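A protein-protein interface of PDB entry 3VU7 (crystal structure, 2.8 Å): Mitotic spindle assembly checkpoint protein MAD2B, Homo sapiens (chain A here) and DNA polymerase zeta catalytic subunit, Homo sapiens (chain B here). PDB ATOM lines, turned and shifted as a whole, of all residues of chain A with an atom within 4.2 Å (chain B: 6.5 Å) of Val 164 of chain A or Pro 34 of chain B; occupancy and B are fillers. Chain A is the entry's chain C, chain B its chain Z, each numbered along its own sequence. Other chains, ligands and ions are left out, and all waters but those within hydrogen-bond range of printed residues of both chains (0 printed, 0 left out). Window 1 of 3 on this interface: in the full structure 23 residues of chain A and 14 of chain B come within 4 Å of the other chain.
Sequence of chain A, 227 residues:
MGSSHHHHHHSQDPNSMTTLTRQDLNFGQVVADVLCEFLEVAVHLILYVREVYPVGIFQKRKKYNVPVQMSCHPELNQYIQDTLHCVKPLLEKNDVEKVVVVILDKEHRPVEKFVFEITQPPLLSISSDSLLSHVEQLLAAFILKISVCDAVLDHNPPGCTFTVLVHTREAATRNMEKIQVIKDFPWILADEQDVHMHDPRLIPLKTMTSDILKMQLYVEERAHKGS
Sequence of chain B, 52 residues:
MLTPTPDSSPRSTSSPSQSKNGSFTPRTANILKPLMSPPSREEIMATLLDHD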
ATOM      1  N   TYR A  79      -9.077  21.060  12.351  1.00  0.00           N
ATOM      2  CA  TYR A  79     -10.393  21.103  11.726  1.00  0.00           C
ATOM      3  C   TYR A  79     -10.516  22.349  10.885  1.00  0.00           C
ATOM      4  O   TYR A  79     -10.814  22.295   9.700  1.00  0.00           O
ATOM      5  CB  TYR A  79     -11.511  21.078  12.776  1.00  0.00           C
ATOM      6  CG  TYR A  79     -12.876  21.120  12.151  1.00  0.00           C
ATOM      7  CD1 TYR A  79     -13.542  19.953  11.841  1.00  0.00           C
ATOM      8  CD2 TYR A  79     -13.507  22.337  11.857  1.00  0.00           C
ATOM      9  CE1 TYR A  79     -14.799  19.981  11.219  1.00  0.00           C
ATOM     10  CE2 TYR A  79     -14.756  22.364  11.253  1.00  0.00           C
ATOM     11  CZ  TYR A  79     -15.404  21.173  10.940  1.00  0.00           C
ATOM     12  OH  TYR A  79     -16.649  21.151  10.348  1.00  0.00           O
ATOM     13  N   THR A  83     -10.707  22.491   6.546  1.00  0.00           N
ATOM     14  CA  THR A  83     -11.708  23.296   5.867  1.00  0.00           C
ATOM     15  C   THR A  83     -11.060  24.311   4.881  1.00  0.00           C
ATOM     16  O   THR A  83     -11.280  24.215   3.647  1.00  0.00           O
ATOM     17  CB  THR A  83     -12.630  23.952   6.887  1.00  0.00           C
ATOM     18  OG1 THR A  83     -12.930  22.991   7.905  1.00  0.00           O
ATOM     19  CG2 THR A  83     -13.909  24.374   6.244  1.00  0.00           C
ATOM     20  N   VAL A 100     -19.383  31.074   4.724  1.00  0.00           N
ATOM     21  CA  VAL A 100     -20.254  31.429   5.824  1.00  0.00           C
ATOM     22  C   VAL A 100     -19.921  30.596   7.049  1.00  0.00           C
ATOM     23  O   VAL A 100     -19.903  29.345   6.976  1.00  0.00           O
ATOM     24  CB  VAL A 100     -21.721  31.083   5.498  1.00  0.00           C
ATOM     25  CG1 VAL A 100     -22.599  31.277   6.731  1.00  0.00           C
ATOM     26  CG2 VAL A 100     -22.238  31.928   4.351  1.00  0.00           C
ATOM     27  N   PHE A 162     -20.590  25.146  15.993  1.00  0.00           N
ATOM     28  CA  PHE A 162     -20.496  25.875  14.730  1.00  0.00           C
ATOM     29  C   PHE A 162     -20.230  24.975  13.547  1.00  0.00           C
ATOM     30  O   PHE A 162     -19.928  23.790  13.730  1.00  0.00           O
ATOM     31  CB  PHE A 162     -19.396  26.907  14.797  1.00  0.00           C
ATOM     32  CG  PHE A 162     -18.072  26.440  14.258  1.00  0.00           C
ATOM     33  CD1 PHE A 162     -17.217  25.663  15.042  1.00  0.00           C
ATOM     34  CD2 PHE A 162     -17.662  26.812  12.997  1.00  0.00           C
ATOM     35  CE1 PHE A 162     -15.974  25.254  14.556  1.00  0.00           C
ATOM     36  CE2 PHE A 162     -16.425  26.401  12.509  1.00  0.00           C
ATOM     37  CZ  PHE A 162     -15.579  25.632  13.294  1.00  0.00           C
ATOM     38  N   THR A 163     -20.306  25.555  12.339  1.00  0.00           N
ATOM     39  CA  THR A 163     -20.035  24.845  11.088  1.00  0.00           C
ATOM     40  C   THR A 163     -19.589  25.809   9.960  1.00  0.00           C
ATOM     41  O   THR A 163     -19.764  27.008  10.101  1.00  0.00           O
ATOM     42  CB  THR A 163     -21.221  23.981  10.633  1.00  0.00           C
ATOM     43  OG1 THR A 163     -20.885  23.428   9.363  1.00  0.00           O
ATOM     44  CG2 THR A 163     -22.469  24.793  10.420  1.00  0.00           C
ATOM     45  N   VAL A 164     -18.984  25.303   8.885  1.00  0.00           N
ATOM     46  CA  VAL A 164     -18.630  26.124   7.749  1.00  0.00           C
ATOM     47  C   VAL A 164     -19.404  25.723   6.470  1.00  0.00           C
ATOM     48  O   VAL A 164     -19.567  24.540   6.164  1.00  0.00           O
ATOM     49  CB  VAL A 164     -17.117  26.071   7.438  1.00  0.00           C
ATOM     50  CG1 VAL A 164     -16.737  27.057   6.315  1.00  0.00           C
ATOM     51  CG2 VAL A 164     -16.326  26.358   8.703  1.00  0.00           C
ATOM     52  N   LEU A 165     -19.886  26.715   5.727  1.00  0.00           N
ATOM     53  CA  LEU A 165     -20.631  26.473   4.492  1.00  0.00           C
ATOM     54  C   LEU A 165     -19.949  27.274   3.406  1.00  0.00           C
ATOM     55  O   LEU A 165     -19.548  28.429   3.623  1.00  0.00           O
ATOM     56  CB  LEU A 165     -22.081  26.949   4.618  1.00  0.00           C
ATOM     57  CG  LEU A 165     -23.017  26.260   5.619  1.00  0.00           C
ATOM     58  CD1 LEU A 165     -24.444  26.761   5.454  1.00  0.00           C
ATOM     59  CD2 LEU A 165     -22.956  24.790   5.326  1.00  0.00           C
ATOM     60  N   PHE A 185     -11.357  13.877   5.111  1.00  0.00           N
ATOM     61  CA  PHE A 185     -12.118  15.109   5.276  1.00  0.00           C
ATOM     62  C   PHE A 185     -13.093  15.446   4.117  1.00  0.00           C
ATOM     63  O   PHE A 185     -13.013  16.507   3.480  1.00  0.00           O
ATOM     64  CB  PHE A 185     -11.188  16.251   5.627  1.00  0.00           C
ATOM     65  CG  PHE A 185     -11.871  17.405   6.323  1.00  0.00           C
ATOM     66  CD1 PHE A 185     -12.007  17.410   7.705  1.00  0.00           C
ATOM     67  CD2 PHE A 185     -12.313  18.544   5.583  1.00  0.00           C
ATOM     68  CE1 PHE A 185     -12.617  18.490   8.346  1.00  0.00           C
ATOM     69  CE2 PHE A 185     -12.881  19.637   6.228  1.00  0.00           C
ATOM     70  CZ  PHE A 185     -13.059  19.602   7.607  1.00  0.00           C
ATOM     71  N   PRO A 186     -14.065  14.559   3.891  1.00  0.00           N
ATOM     72  CA  PRO A 186     -15.012  14.723   2.820  1.00  0.00           C
ATOM     73  C   PRO A 186     -15.941  15.955   2.962  1.00  0.00           C
ATOM     74  O   PRO A 186     -16.169  16.413   4.092  1.00  0.00           O
ATOM     75  CB  PRO A 186     -15.858  13.444   2.917  1.00  0.00           C
ATOM     76  CG  PRO A 186     -15.127  12.538   3.805  1.00  0.00           C
ATOM     77  CD  PRO A 186     -14.410  13.410   4.744  1.00  0.00           C
ATOM     78  N   TRP A 187     -16.468  16.438   1.823  1.00  0.00           N
ATOM     79  CA  TRP A 187     -17.574  17.394   1.770  1.00  0.00           C
ATOM     80  C   TRP A 187     -18.833  16.789   1.207  1.00  0.00           C
ATOM     81  O   TRP A 187     -18.763  15.955   0.311  1.00  0.00           O
ATOM     82  CB  TRP A 187     -17.198  18.632   0.937  1.00  0.00           C
ATOM     83  CG  TRP A 187     -16.127  19.437   1.597  1.00  0.00           C
ATOM     84  CD1 TRP A 187     -14.813  19.049   1.875  1.00  0.00           C
ATOM     85  CD2 TRP A 187     -16.245  20.799   2.144  1.00  0.00           C
ATOM     86  NE1 TRP A 187     -14.104  20.068   2.496  1.00  0.00           N
ATOM     87  CE2 TRP A 187     -14.906  21.142   2.698  1.00  0.00           C
ATOM     88  CE3 TRP A 187     -17.288  21.726   2.262  1.00  0.00           C
ATOM     89  CZ2 TRP A 187     -14.655  22.358   3.292  1.00  0.00           C
ATOM     90  CZ3 TRP A 187     -17.013  22.956   2.878  1.00  0.00           C
ATOM     91  CH2 TRP A 187     -15.726  23.267   3.359  1.00  0.00           C
ATOM     92  N   LEU B  32     -21.741  23.819  -0.190  1.00  0.00           N
ATOM     93  CA  LEU B  32     -20.952  22.695   0.305  1.00  0.00           C
ATOM     94  C   LEU B  32     -20.644  22.772   1.766  1.00  0.00           C
ATOM     95  O   LEU B  32     -20.468  23.831   2.325  1.00  0.00           O
ATOM     96  CB  LEU B  32     -19.650  22.581  -0.462  1.00  0.00           C
ATOM     97  CG  LEU B  32     -19.837  22.327  -1.944  1.00  0.00           C
ATOM     98  CD1 LEU B  32     -18.519  22.403  -2.681  1.00  0.00           C
ATOM     99  CD2 LEU B  32     -20.438  20.961  -2.133  1.00  0.00           C
ATOM    100  N   LYS B  33     -20.513  21.611   2.363  1.00  0.00           N
ATOM    101  CA  LYS B  33     -20.427  21.470   3.801  1.00  0.00           C
ATOM    102  C   LYS B  33     -19.443  20.333   4.016  1.00  0.00           C
ATOM    103  O   LYS B  33     -19.412  19.423   3.196  1.00  0.00           O
ATOM    104  CB  LYS B  33     -21.824  21.088   4.306  1.00  0.00           C
ATOM    105  CG  LYS B  33     -22.033  20.861   5.778  1.00  0.00           C
ATOM    106  CD  LYS B  33     -23.249  19.947   5.926  1.00  0.00           C
ATOM    107  CE  LYS B  33     -23.630  19.553   7.366  1.00  0.00           C
ATOM    108  NZ  LYS B  33     -22.568  18.997   8.280  1.00  0.00           N
ATOM    109  N   PRO B  34     -18.616  20.387   5.092  1.00  0.00           N
ATOM    110  CA  PRO B  34     -17.824  19.244   5.464  1.00  0.00           C
ATOM    111  C   PRO B  34     -18.737  18.235   6.086  1.00  0.00           C
ATOM    112  O   PRO B  34     -19.756  18.610   6.650  1.00  0.00           O
ATOM    113  CB  PRO B  34     -16.896  19.804   6.530  1.00  0.00           C
ATOM    114  CG  PRO B  34     -16.800  21.234   6.230  1.00  0.00           C
ATOM    115  CD  PRO B  34     -18.224  21.547   5.897  1.00  0.00           C
ATOM    116  N   LEU B  35     -18.387  16.958   5.974  1.00  0.00           N
ATOM    117  CA  LEU B  35     -19.180  15.905   6.555  1.00  0.00           C
ATOM    118  C   LEU B  35     -18.849  15.834   8.033  1.00  0.00           C
ATOM    119  O   LEU B  35     -19.726  15.608   8.850  1.00  0.00           O
ATOM    120  CB  LEU B  35     -18.887  14.575   5.872  1.00  0.00           C
ATOM    121  CG  LEU B  35     -19.405  13.274   6.491  1.00  0.00           C
ATOM    122  CD1 LEU B  35     -20.812  12.945   6.063  1.00  0.00           C
ATOM    123  CD2 LEU B  35     -18.488  12.146   6.095  1.00  0.00           C
ATOM    124  N   MET B  36     -17.585  16.062   8.369  1.00  0.00           N
ATOM    125  CA  MET B  36     -17.088  15.912   9.729  1.00  0.00           C
ATOM    126  C   MET B  36     -17.461  17.099  10.554  1.00  0.00           C
ATOM    127  O   MET B  36     -17.504  18.211  10.067  1.00  0.00           O
ATOM    128  CB  MET B  36     -15.578  15.746   9.729  1.00  0.00           C
ATOM    129  CG  MET B  36     -15.125  14.448   9.086  1.00  0.00           C
ATOM    130  SD  MET B  36     -15.559  13.013  10.088  1.00  0.00           S
ATOM    131  CE  MET B  36     -15.946  11.809   8.815  1.00  0.00           C
ATOM    132  N   SER B  37     -17.739  16.858  11.822  1.00  0.00           N
ATOM    133  CA  SER B  37     -18.064  17.935  12.725  1.00  0.00           C
ATOM    134  C   SER B  37     -16.838  18.431  13.461  1.00  0.00           C
ATOM    135  O   SER B  37     -15.901  17.669  13.713  1.00  0.00           O
ATOM    136  CB  SER B  37     -19.141  17.497  13.693  1.00  0.00           C
ATOM    137  OG  SER B  37     -20.374  17.776  13.098  1.00  0.00           O
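OH of Tyr 79 of chain A sits at hydrogen-bond distance from O of Met 36 of chain B, at 3.1 Å. The backbone NH (N) of Leu 35 of chain B sits at hydrogen-bond distance from the backbone carbonyl oxygen (O) of Pro 186 of chain A, at 3.0 Å.
O of Tyr 79 of chain A lies within hydrogen-bond range of OG1 of Thr 83 of chain A (2.9 Å). The backbone carbonyl oxygen (O) of Leu 165 of chain A lies within hydrogen-bond range of the backbone NH (N) of Val 100 of chain A (2.9 Å).
Among the printed residues, pairs that only touch across the chains: Trp 187 of chain A with Lys 33 of chain B, Val 164 of chain A with Pro 34 of chain B, Trp 187 of chain A with Pro 34 of chain B, Tyr 79 of chain A with Ser 37 of chain B, Leu 165 of chain A with Leu 32 of chain B, Trp 187 of chain A with Leu 32 of chain B, Pro 186 of chain A with Pro 34 of chain B, Val 164 of chain A with Lys 33 of chain B and Phe 185 of chain A with Pro 34 of chain B.
Of the printed residues of chain B, Val 164 of chain A touches Lys 33 (3.97 Å) and Pro 34 (3.3 Å). Printed residues of chain A within 4 Å of Pro 34 of chain B: Val 164, Phe 185, Pro 186 and Trp 187. Printed residues of chain B within 4 Å of Trp 187 of chain A: Leu 32, Lys 33 and Pro 34. Printed residues of chain A within 4 Å of Lys 33 of chain B: Val 164 and Trp 187. The nearest printed residue of chain A that does not touch Pro 34 of chain B is Tyr 79 of chain A (4.1 Å).
Hydrophobic or aromatic side chains of chain B within 4 Å of the printed part of chain A: Leu 32, Pro 34 and Leu 35. Of the 10 printed residues of chain A, 6 touch a printed residue of chain B. Printed residues of chain A that touch a printed residue of chain B: Tyr 79, Val 164, Leu 165, Phe 185, Pro 186 and Trp 187. Among the printed residues, no Asp or Glu carboxylate lies within 4 Å of a Lys or Arg side-chain nitrogen of the other chain.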
